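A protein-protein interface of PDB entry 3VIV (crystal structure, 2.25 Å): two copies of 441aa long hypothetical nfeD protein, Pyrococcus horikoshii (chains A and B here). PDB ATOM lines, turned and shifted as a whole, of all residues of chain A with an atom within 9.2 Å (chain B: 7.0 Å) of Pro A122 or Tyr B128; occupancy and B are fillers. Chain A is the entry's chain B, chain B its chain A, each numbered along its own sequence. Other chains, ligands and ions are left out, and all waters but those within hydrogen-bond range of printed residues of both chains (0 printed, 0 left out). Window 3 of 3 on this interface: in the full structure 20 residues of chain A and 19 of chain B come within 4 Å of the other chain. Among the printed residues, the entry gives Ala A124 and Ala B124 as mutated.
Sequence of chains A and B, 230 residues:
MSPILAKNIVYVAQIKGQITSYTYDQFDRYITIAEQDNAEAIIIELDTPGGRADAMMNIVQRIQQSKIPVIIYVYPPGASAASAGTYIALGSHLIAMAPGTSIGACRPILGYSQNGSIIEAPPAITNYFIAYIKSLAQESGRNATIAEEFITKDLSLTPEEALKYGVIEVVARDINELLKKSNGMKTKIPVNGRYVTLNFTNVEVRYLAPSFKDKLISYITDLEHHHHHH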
ATOM      1  N   PRO A 108      33.208 -19.035  -1.985  1.00  0.00           N
ATOM      2  CA  PRO A 108      31.986 -19.792  -1.675  1.00  0.00           C
ATOM      3  C   PRO A 108      32.272 -21.272  -1.412  1.00  0.00           C
ATOM      4  O   PRO A 108      33.209 -21.840  -1.992  1.00  0.00           O
ATOM      5  CB  PRO A 108      31.115 -19.622  -2.929  1.00  0.00           C
ATOM      6  CG  PRO A 108      32.047 -19.125  -4.017  1.00  0.00           C
ATOM      7  CD  PRO A 108      33.180 -18.429  -3.331  1.00  0.00           C
ATOM      8  N   ILE A 109      31.505 -21.853  -0.489  1.00  0.00           N
ATOM      9  CA  ILE A 109      31.455 -23.295  -0.252  1.00  0.00           C
ATOM     10  C   ILE A 109      29.984 -23.701  -0.185  1.00  0.00           C
ATOM     11  O   ILE A 109      29.135 -22.892   0.173  1.00  0.00           O
ATOM     12  CB  ILE A 109      32.132 -23.712   1.079  1.00  0.00           C
ATOM     13  CG1 ILE A 109      31.481 -22.969   2.269  1.00  0.00           C
ATOM     14  CG2 ILE A 109      33.680 -23.568   0.977  1.00  0.00           C
ATOM     15  CD1 ILE A 109      31.826 -23.503   3.637  1.00  0.00           C
ATOM     16  N   LEU A 110      29.677 -24.947  -0.534  1.00  0.00           N
ATOM     17  CA  LEU A 110      28.310 -25.433  -0.404  1.00  0.00           C
ATOM     18  C   LEU A 110      27.913 -25.432   1.065  1.00  0.00           C
ATOM     19  O   LEU A 110      26.750 -25.228   1.385  1.00  0.00           O
ATOM     20  CB  LEU A 110      28.129 -26.806  -1.045  1.00  0.00           C
ATOM     21  CG  LEU A 110      28.027 -26.826  -2.575  1.00  0.00           C
ATOM     22  CD1 LEU A 110      27.727 -28.231  -3.086  1.00  0.00           C
ATOM     23  CD2 LEU A 110      26.963 -25.863  -3.065  1.00  0.00           C
ATOM     24  N   GLY A 111      28.894 -25.614   1.948  1.00  0.00           N
ATOM     25  CA  GLY A 111      28.686 -25.498   3.392  1.00  0.00           C
ATOM     26  C   GLY A 111      29.657 -26.336   4.201  1.00  0.00           C
ATOM     27  O   GLY A 111      30.588 -26.911   3.655  1.00  0.00           O
ATOM     28  N   ILE A 118      34.633 -29.523   4.921  1.00  0.00           N
ATOM     29  CA  ILE A 118      33.821 -28.541   4.190  1.00  0.00           C
ATOM     30  C   ILE A 118      33.346 -29.128   2.854  1.00  0.00           C
ATOM     31  O   ILE A 118      34.030 -29.971   2.251  1.00  0.00           O
ATOM     32  CB  ILE A 118      34.526 -27.157   3.982  1.00  0.00           C
ATOM     33  CG1 ILE A 118      35.548 -27.194   2.845  1.00  0.00           C
ATOM     34  CG2 ILE A 118      35.140 -26.624   5.290  1.00  0.00           C
ATOM     35  CD1 ILE A 118      36.072 -25.785   2.460  1.00  0.00           C
ATOM     36  N   ILE A 119      32.159 -28.707   2.419  1.00  0.00           N
ATOM     37  CA  ILE A 119      31.617 -29.151   1.140  1.00  0.00           C
ATOM     38  C   ILE A 119      32.029 -28.135   0.078  1.00  0.00           C
ATOM     39  O   ILE A 119      31.670 -26.966   0.162  1.00  0.00           O
ATOM     40  CB  ILE A 119      30.070 -29.326   1.171  1.00  0.00           C
ATOM     41  CG1 ILE A 119      29.612 -29.963   2.493  1.00  0.00           C
ATOM     42  CG2 ILE A 119      29.614 -30.151  -0.024  1.00  0.00           C
ATOM     43  CD1 ILE A 119      28.158 -29.644   2.905  1.00  0.00           C
ATOM     44  N   GLU A 120      32.793 -28.601  -0.905  1.00  0.00           N
ATOM     45  CA  GLU A 120      33.354 -27.747  -1.946  1.00  0.00           C
ATOM     46  C   GLU A 120      32.283 -27.214  -2.890  1.00  0.00           C
ATOM     47  O   GLU A 120      31.383 -27.949  -3.297  1.00  0.00           O
ATOM     48  CB  GLU A 120      34.412 -28.518  -2.746  1.00  0.00           C
ATOM     49  CG  GLU A 120      35.318 -27.647  -3.621  1.00  0.00           C
ATOM     50  CD  GLU A 120      36.484 -28.425  -4.233  1.00  0.00           C
ATOM     51  OE1 GLU A 120      36.258 -29.488  -4.859  1.00  0.00           O
ATOM     52  OE2 GLU A 120      37.634 -27.956  -4.095  1.00  0.00           O
ATOM     53  N   ALA A 121      32.392 -25.937  -3.237  1.00  0.00           N
ATOM     54  CA  ALA A 121      31.524 -25.345  -4.242  1.00  0.00           C
ATOM     55  C   ALA A 121      32.039 -25.698  -5.626  1.00  0.00           C
ATOM     56  O   ALA A 121      33.254 -25.625  -5.878  1.00  0.00           O
ATOM     57  CB  ALA A 121      31.458 -23.839  -4.072  1.00  0.00           C
ATOM     58  N   PRO A 122      31.125 -26.095  -6.535  1.00  0.00           N
ATOM     59  CA  PRO A 122      31.530 -26.396  -7.911  1.00  0.00           C
ATOM     60  C   PRO A 122      32.028 -25.129  -8.613  1.00  0.00           C
ATOM     61  O   PRO A 122      31.562 -24.031  -8.282  1.00  0.00           O
ATOM     62  CB  PRO A 122      30.234 -26.903  -8.562  1.00  0.00           C
ATOM     63  CG  PRO A 122      29.304 -27.206  -7.429  1.00  0.00           C
ATOM     64  CD  PRO A 122      29.675 -26.274  -6.336  1.00  0.00           C
ATOM     65  N   PRO A 123      32.968 -25.275  -9.576  1.00  0.00           N
ATOM     66  CA  PRO A 123      33.561 -24.112 -10.257  1.00  0.00           C
ATOM     67  C   PRO A 123      32.537 -23.068 -10.746  1.00  0.00           C
ATOM     68  O   PRO A 123      32.828 -21.863 -10.709  1.00  0.00           O
ATOM     69  CB  PRO A 123      34.303 -24.734 -11.436  1.00  0.00           C
ATOM     70  CG  PRO A 123      34.636 -26.124 -10.976  1.00  0.00           C
ATOM     71  CD  PRO A 123      33.512 -26.554 -10.081  1.00  0.00           C
ATOM     72  N   ALA A 124      31.354 -23.526 -11.169  1.00  0.00           N
ATOM     73  CA  ALA A 124      30.300 -22.646 -11.687  1.00  0.00           C
ATOM     74  C   ALA A 124      29.832 -21.621 -10.654  1.00  0.00           C
ATOM     75  O   ALA A 124      29.795 -20.429 -10.945  1.00  0.00           O
ATOM     76  CB  ALA A 124      29.118 -23.457 -12.222  1.00  0.00           C
ATOM     77  N   ILE A 125      29.483 -22.091  -9.458  1.00  0.00           N
ATOM     78  CA  ILE A 125      29.187 -21.220  -8.318  1.00  0.00           C
ATOM     79  C   ILE A 125      30.322 -20.240  -8.010  1.00  0.00           C
ATOM     80  O   ILE A 125      30.085 -19.068  -7.736  1.00  0.00           O
ATOM     81  CB  ILE A 125      28.856 -22.050  -7.049  1.00  0.00           C
ATOM     82  CG1 ILE A 125      27.530 -22.809  -7.218  1.00  0.00           C
ATOM     83  CG2 ILE A 125      28.841 -21.167  -5.809  1.00  0.00           C
ATOM     84  CD1 ILE A 125      26.275 -21.911  -7.388  1.00  0.00           C
ATOM     85  N   THR A 126      31.551 -20.725  -8.058  1.00  0.00           N
ATOM     86  CA  THR A 126      32.720 -19.891  -7.803  1.00  0.00           C
ATOM     87  C   THR A 126      32.818 -18.777  -8.851  1.00  0.00           C
ATOM     88  O   THR A 126      32.883 -17.600  -8.494  1.00  0.00           O
ATOM     89  CB  THR A 126      34.001 -20.755  -7.734  1.00  0.00           C
ATOM     90  OG1 THR A 126      33.839 -21.741  -6.704  1.00  0.00           O
ATOM     91  CG2 THR A 126      35.253 -19.901  -7.456  1.00  0.00           C
ATOM     92  N   ASN A 127      32.785 -19.155 -10.132  1.00  0.00           N
ATOM     93  CA  ASN A 127      32.816 -18.194 -11.241  1.00  0.00           C
ATOM     94  C   ASN A 127      31.653 -17.215 -11.166  1.00  0.00           C
ATOM     95  O   ASN A 127      31.820 -16.026 -11.420  1.00  0.00           O
ATOM     96  CB  ASN A 127      32.801 -18.907 -12.605  1.00  0.00           C
ATOM     97  CG  ASN A 127      34.049 -19.749 -12.847  1.00  0.00           C
ATOM     98  OD1 ASN A 127      35.142 -19.429 -12.364  1.00  0.00           O
ATOM     99  ND2 ASN A 127      33.889 -20.833 -13.598  1.00  0.00           N
ATOM    100  N   TYR A 128      30.478 -17.722 -10.811  1.00  0.00           N
ATOM    101  CA  TYR A 128      29.303 -16.881 -10.657  1.00  0.00           C
ATOM    102  C   TYR A 128      29.540 -15.799  -9.587  1.00  0.00           C
ATOM    103  O   TYR A 128      29.177 -14.632  -9.793  1.00  0.00           O
ATOM    104  CB  TYR A 128      28.098 -17.748 -10.310  1.00  0.00           C
ATOM    105  CG  TYR A 128      26.798 -17.022 -10.037  1.00  0.00           C
ATOM    106  CD1 TYR A 128      25.794 -16.953 -11.011  1.00  0.00           C
ATOM    107  CD2 TYR A 128      26.551 -16.441  -8.798  1.00  0.00           C
ATOM    108  CE1 TYR A 128      24.580 -16.307 -10.748  1.00  0.00           C
ATOM    109  CE2 TYR A 128      25.356 -15.790  -8.532  1.00  0.00           C
ATOM    110  CZ  TYR A 128      24.377 -15.730  -9.509  1.00  0.00           C
ATOM    111  OH  TYR A 128      23.189 -15.094  -9.224  1.00  0.00           O
ATOM    112  N   PHE A 129      30.159 -16.174  -8.463  1.00  0.00           N
ATOM    113  CA  PHE A 129      30.430 -15.188  -7.414  1.00  0.00           C
ATOM    114  C   PHE A 129      31.590 -14.266  -7.705  1.00  0.00           C
ATOM    115  O   PHE A 129      31.562 -13.119  -7.277  1.00  0.00           O
ATOM    116  CB  PHE A 129      30.460 -15.812  -6.024  1.00  0.00           C
ATOM    117  CG  PHE A 129      29.084 -16.190  -5.547  1.00  0.00           C
ATOM    118  CD1 PHE A 129      28.540 -17.421  -5.871  1.00  0.00           C
ATOM    119  CD2 PHE A 129      28.303 -15.266  -4.869  1.00  0.00           C
ATOM    120  CE1 PHE A 129      27.244 -17.753  -5.474  1.00  0.00           C
ATOM    121  CE2 PHE A 129      27.010 -15.579  -4.459  1.00  0.00           C
ATOM    122  CZ  PHE A 129      26.474 -16.834  -4.761  1.00  0.00           C
ATOM    123  N   ILE A 130      32.578 -14.749  -8.460  1.00  0.00           N
ATOM    124  CA  ILE A 130      33.639 -13.880  -8.971  1.00  0.00           C
ATOM    125  C   ILE A 130      33.017 -12.785  -9.830  1.00  0.00           C
ATOM    126  O   ILE A 130      33.308 -11.622  -9.610  1.00  0.00           O
ATOM    127  CB  ILE A 130      34.739 -14.651  -9.760  1.00  0.00           C
ATOM    128  CG1 ILE A 130      35.603 -15.497  -8.816  1.00  0.00           C
ATOM    129  CG2 ILE A 130      35.651 -13.684 -10.557  1.00  0.00           C
ATOM    130  CD1 ILE A 130      36.388 -16.638  -9.538  1.00  0.00           C
ATOM    131  N   MET B  57      22.706 -32.399   2.696  1.00  0.00           N
ATOM    132  CA  MET B  57      23.878 -33.242   2.445  1.00  0.00           C
ATOM    133  C   MET B  57      24.487 -33.795   3.728  1.00  0.00           C
ATOM    134  O   MET B  57      24.930 -34.952   3.747  1.00  0.00           O
ATOM    135  CB  MET B  57      24.931 -32.528   1.586  1.00  0.00           C
ATOM    136  CG  MET B  57      24.409 -32.172   0.205  1.00  0.00           C
ATOM    137  SD  MET B  57      25.651 -31.361  -0.810  1.00  0.00           S
ATOM    138  CE  MET B  57      24.664 -30.173  -1.668  1.00  0.00           C
ATOM    139  N   PRO B 108      17.202 -27.555  -7.790  1.00  0.00           N
ATOM    140  CA  PRO B 108      17.972 -26.612  -6.962  1.00  0.00           C
ATOM    141  C   PRO B 108      17.760 -25.174  -7.397  1.00  0.00           C
ATOM    142  O   PRO B 108      17.595 -24.915  -8.592  1.00  0.00           O
ATOM    143  CB  PRO B 108      19.427 -27.001  -7.223  1.00  0.00           C
ATOM    144  CG  PRO B 108      19.401 -27.684  -8.566  1.00  0.00           C
ATOM    145  CD  PRO B 108      18.077 -28.405  -8.620  1.00  0.00           C
ATOM    146  N   PRO B 123      22.952 -23.031 -14.871  1.00  0.00           N
ATOM    147  CA  PRO B 123      22.667 -24.354 -15.416  1.00  0.00           C
ATOM    148  C   PRO B 123      23.563 -25.456 -14.827  1.00  0.00           C
ATOM    149  O   PRO B 123      23.069 -26.532 -14.530  1.00  0.00           O
ATOM    150  CB  PRO B 123      22.929 -24.182 -16.922  1.00  0.00           C
ATOM    151  CG  PRO B 123      22.675 -22.735 -17.172  1.00  0.00           C
ATOM    152  CD  PRO B 123      23.161 -22.030 -15.940  1.00  0.00           C
ATOM    153  N   ALA B 124      24.849 -25.165 -14.631  1.00  0.00           N
ATOM    154  CA  ALA B 124      25.820 -26.170 -14.195  1.00  0.00           C
ATOM    155  C   ALA B 124      25.590 -26.673 -12.771  1.00  0.00           C
ATOM    156  O   ALA B 124      25.981 -27.793 -12.436  1.00  0.00           O
ATOM    157  CB  ALA B 124      27.256 -25.662 -14.382  1.00  0.00           C
ATOM    158  N   ILE B 125      24.924 -25.875 -11.947  1.00  0.00           N
ATOM    159  CA  ILE B 125      24.571 -26.327 -10.605  1.00  0.00           C
ATOM    160  C   ILE B 125      23.345 -27.271 -10.586  1.00  0.00           C
ATOM    161  O   ILE B 125      23.267 -28.201  -9.772  1.00  0.00           O
ATOM    162  CB  ILE B 125      24.490 -25.149  -9.602  1.00  0.00           C
ATOM    163  CG1 ILE B 125      23.712 -25.539  -8.350  1.00  0.00           C
ATOM    164  CG2 ILE B 125      23.877 -23.962 -10.234  1.00  0.00           C
ATOM    165  CD1 ILE B 125      24.486 -25.222  -7.111  1.00  0.00           C
ATOM    166  N   THR B 126      22.414 -27.045 -11.508  1.00  0.00           N
ATOM    167  CA  THR B 126      21.375 -28.023 -11.793  1.00  0.00           C
ATOM    168  C   THR B 126      22.023 -29.378 -12.124  1.00  0.00           C
ATOM    169  O   THR B 126      21.683 -30.407 -11.500  1.00  0.00           O
ATOM    170  CB  THR B 126      20.441 -27.521 -12.914  1.00  0.00           C
ATOM    171  OG1 THR B 126      19.757 -26.350 -12.454  1.00  0.00           O
ATOM    172  CG2 THR B 126      19.416 -28.569 -13.314  1.00  0.00           C
ATOM    173  N   ASN B 127      22.976 -29.374 -13.064  1.00  0.00           N
ATOM    174  CA  ASN B 127      23.711 -30.595 -13.441  1.00  0.00           C
ATOM    175  C   ASN B 127      24.417 -31.273 -12.243  1.00  0.00           C
ATOM    176  O   ASN B 127      24.423 -32.504 -12.127  1.00  0.00           O
ATOM    177  CB  ASN B 127      24.702 -30.315 -14.585  1.00  0.00           C
ATOM    178  CG  ASN B 127      24.006 -29.948 -15.910  1.00  0.00           C
ATOM    179  OD1 ASN B 127      22.856 -30.325 -16.158  1.00  0.00           O
ATOM    180  ND2 ASN B 127      24.725 -29.229 -16.774  1.00  0.00           N
ATOM    181  N   TYR B 128      24.980 -30.458 -11.351  1.00  0.00           N
ATOM    182  CA  TYR B 128      25.591 -30.961 -10.121  1.00  0.00           C
ATOM    183  C   TYR B 128      24.581 -31.711  -9.219  1.00  0.00           C
ATOM    184  O   TYR B 128      24.868 -32.804  -8.722  1.00  0.00           O
ATOM    185  CB  TYR B 128      26.301 -29.819  -9.366  1.00  0.00           C
ATOM    186  CG  TYR B 128      26.878 -30.216  -8.028  1.00  0.00           C
ATOM    187  CD1 TYR B 128      28.248 -30.466  -7.875  1.00  0.00           C
ATOM    188  CD2 TYR B 128      26.059 -30.359  -6.922  1.00  0.00           C
ATOM    189  CE1 TYR B 128      28.779 -30.835  -6.634  1.00  0.00           C
ATOM    190  CE2 TYR B 128      26.573 -30.735  -5.695  1.00  0.00           C
ATOM    191  CZ  TYR B 128      27.935 -30.964  -5.561  1.00  0.00           C
ATOM    192  OH  TYR B 128      28.411 -31.336  -4.329  1.00  0.00           O
ATOM    193  N   PHE B 129      23.405 -31.133  -9.006  1.00  0.00           N
ATOM    194  CA  PHE B 129      22.378 -31.831  -8.226  1.00  0.00           C
ATOM    195  C   PHE B 129      21.712 -33.016  -8.936  1.00  0.00           C
ATOM    196  O   PHE B 129      21.239 -33.940  -8.276  1.00  0.00           O
ATOM    197  CB  PHE B 129      21.354 -30.852  -7.675  1.00  0.00           C
ATOM    198  CG  PHE B 129      21.844 -30.131  -6.468  1.00  0.00           C
ATOM    199  CD1 PHE B 129      22.623 -28.989  -6.599  1.00  0.00           C
ATOM    200  CD2 PHE B 129      21.607 -30.646  -5.196  1.00  0.00           C
ATOM    201  CE1 PHE B 129      23.113 -28.338  -5.474  1.00  0.00           C
ATOM    202  CE2 PHE B 129      22.092 -30.000  -4.085  1.00  0.00           C
ATOM    203  CZ  PHE B 129      22.842 -28.839  -4.221  1.00  0.00           C
ATOM    204  N   ILE B 130      21.691 -32.994 -10.265  1.00  0.00           N
ATOM    205  CA  ILE B 130      21.220 -34.138 -11.037  1.00  0.00           C
ATOM    206  C   ILE B 130      22.162 -35.296 -10.743  1.00  0.00           C
ATOM    207  O   ILE B 130      21.704 -36.382 -10.362  1.00  0.00           O
ATOM    208  CB  ILE B 130      21.129 -33.834 -12.565  1.00  0.00           C
ATOM    209  CG1 ILE B 130      19.959 -32.885 -12.842  1.00  0.00           C
ATOM    210  CG2 ILE B 130      20.979 -35.132 -13.381  1.00  0.00           C
ATOM    211  CD1 ILE B 130      19.885 -32.363 -14.301  1.00  0.00           C
ATOM    212  N   ALA B 131      23.471 -35.041 -10.863  1.00  0.00           N
ATOM    213  CA  ALA B 131      24.496 -36.042 -10.556  1.00  0.00           C
ATOM    214  C   ALA B 131      24.335 -36.583  -9.131  1.00  0.00           C
ATOM    215  O   ALA B 131      24.252 -37.805  -8.925  1.00  0.00           O
ATOM    216  CB  ALA B 131      25.897 -35.460 -10.772  1.00  0.00           C
ATOM    217  N   TYR B 132      24.252 -35.679  -8.156  1.00  0.00           N
ATOM    218  CA  TYR B 132      24.070 -36.048  -6.754  1.00  0.00           C
ATOM    219  C   TYR B 132      22.823 -36.936  -6.532  1.00  0.00           C
ATOM    220  O   TYR B 132      22.894 -37.988  -5.884  1.00  0.00           O
ATOM    221  CB  TYR B 132      24.031 -34.775  -5.867  1.00  0.00           C
ATOM    222  CG  TYR B 132      23.944 -35.048  -4.373  1.00  0.00           C
ATOM    223  CD1 TYR B 132      25.027 -35.588  -3.678  1.00  0.00           C
ATOM    224  CD2 TYR B 132      22.799 -34.741  -3.654  1.00  0.00           C
ATOM    225  CE1 TYR B 132      24.961 -35.839  -2.327  1.00  0.00           C
ATOM    226  CE2 TYR B 132      22.724 -35.001  -2.278  1.00  0.00           C
ATOM    227  CZ  TYR B 132      23.806 -35.538  -1.628  1.00  0.00           C
ATOM    228  OH  TYR B 132      23.739 -35.814  -0.286  1.00  0.00           O
ATOM    229  N   ILE B 133      21.684 -36.520  -7.080  1.00  0.00           N
ATOM    230  CA  ILE B 133      20.449 -37.287  -6.901  1.00  0.00           C
ATOM    231  C   ILE B 133      20.501 -38.635  -7.634  1.00  0.00           C
ATOM    232  O   ILE B 133      20.005 -39.636  -7.110  1.00  0.00           O
ATOM    233  CB  ILE B 133      19.175 -36.484  -7.278  1.00  0.00           C
ATOM    234  CG1 ILE B 133      17.994 -36.938  -6.401  1.00  0.00           C
ATOM    235  CG2 ILE B 133      18.867 -36.587  -8.788  1.00  0.00           C
ATOM    236  CD1 ILE B 133      16.728 -36.081  -6.569  1.00  0.00           C
ATOM    237  N   LYS B 134      21.114 -38.658  -8.826  1.00  0.00           N
ATOM    238  CA  LYS B 134      21.340 -39.915  -9.563  1.00  0.00           C
ATOM    239  C   LYS B 134      22.227 -40.870  -8.755  1.00  0.00           C
ATOM    240  O   LYS B 134      21.946 -42.086  -8.689  1.00  0.00           O
ATOM    241  CB  LYS B 134      21.938 -39.642 -10.940  1.00  0.00           C
ATOM    242  CG  LYS B 134      20.923 -39.066 -11.937  1.00  0.00           C
ATOM    243  CD  LYS B 134      21.449 -39.079 -13.377  1.00  0.00           C
ATOM    244  CE  LYS B 134      21.078 -40.367 -14.087  1.00  0.00           C
ATOM    245  NZ  LYS B 134      19.608 -40.447 -14.427  1.00  0.00           N
ATOM    246  N   ILE B 151      14.011 -33.319 -10.606  1.00  0.00           N
ATOM    247  CA  ILE B 151      14.667 -32.033 -10.885  1.00  0.00           C
ATOM    248  C   ILE B 151      14.272 -31.471 -12.257  1.00  0.00           C
ATOM    249  O   ILE B 151      13.779 -30.340 -12.350  1.00  0.00           O
ATOM    250  CB  ILE B 151      16.204 -32.187 -10.813  1.00  0.00           C
ATOM    251  CG1 ILE B 151      16.629 -32.556  -9.379  1.00  0.00           C
ATOM    252  CG2 ILE B 151      16.910 -30.938 -11.336  1.00  0.00           C
ATOM    253  CD1 ILE B 151      18.081 -32.989  -9.226  1.00  0.00           C
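Leu A110 touches Met B57.
CD1 of Leu A110 touches OH of Tyr B128, at 3.4 Å.
Pro A122 touches Tyr B128 (CG to CD1, 3.5 Å).
Ala B124 touches Ala A124.
Ile A125 touches Ile B125 (CD1 to CD1, 3.8 Å).
The backbone NH (N) of Leu A110 lies within hydrogen-bond range of the backbone carbonyl oxygen (O) of Ile A119 (2.9 Å).
Ala B124 touches its own counterpart, Ala A124.
Ile A125 touches its own counterpart, Ile B125.
Positions printed for both chains: 108, 123, 124, 125, 126, 127, 128, 129 and 130.
Of the 5 pairs that touch across the chains among the printed residues, 2 have their exchanged pair printed and touching as well.
Printed residues of chain B within 4 Å of Leu A110: Met B57 and Tyr B128.
Pro A122 touches just one residue of chain B: Tyr B128.
Of the printed residues of chain A, Ala B124 touches Ala A124.
Of the printed residues of chain A, Tyr B128 touches Leu A110 (3.4 Å) and Pro A122 (3.5 Å).
No residue of chain A comes within 4 Å of Ala B131.
Tyr B132 touches none of the printed residues of chain A.
Of the 17 printed residues of chain A, 4 touch a printed residue of chain B.
Printed residues of chain A that touch a printed residue of chain B: Leu A110, Pro A122, Ala A124 and Ile A125.
Hydrophobic or aromatic side chains of chain A that line the printed part of chain B: Leu A110, Pro A122, Ala A124 and Ile A125.
Printed residues of chain B that touch a printed residue of chain A: Met B57, Ala B124, Ile B125 and Tyr B128.
Among the printed residues, no Asp or Glu carboxylate lies within 4 Å of a Lys or Arg side-chain nitrogen of the other chain.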
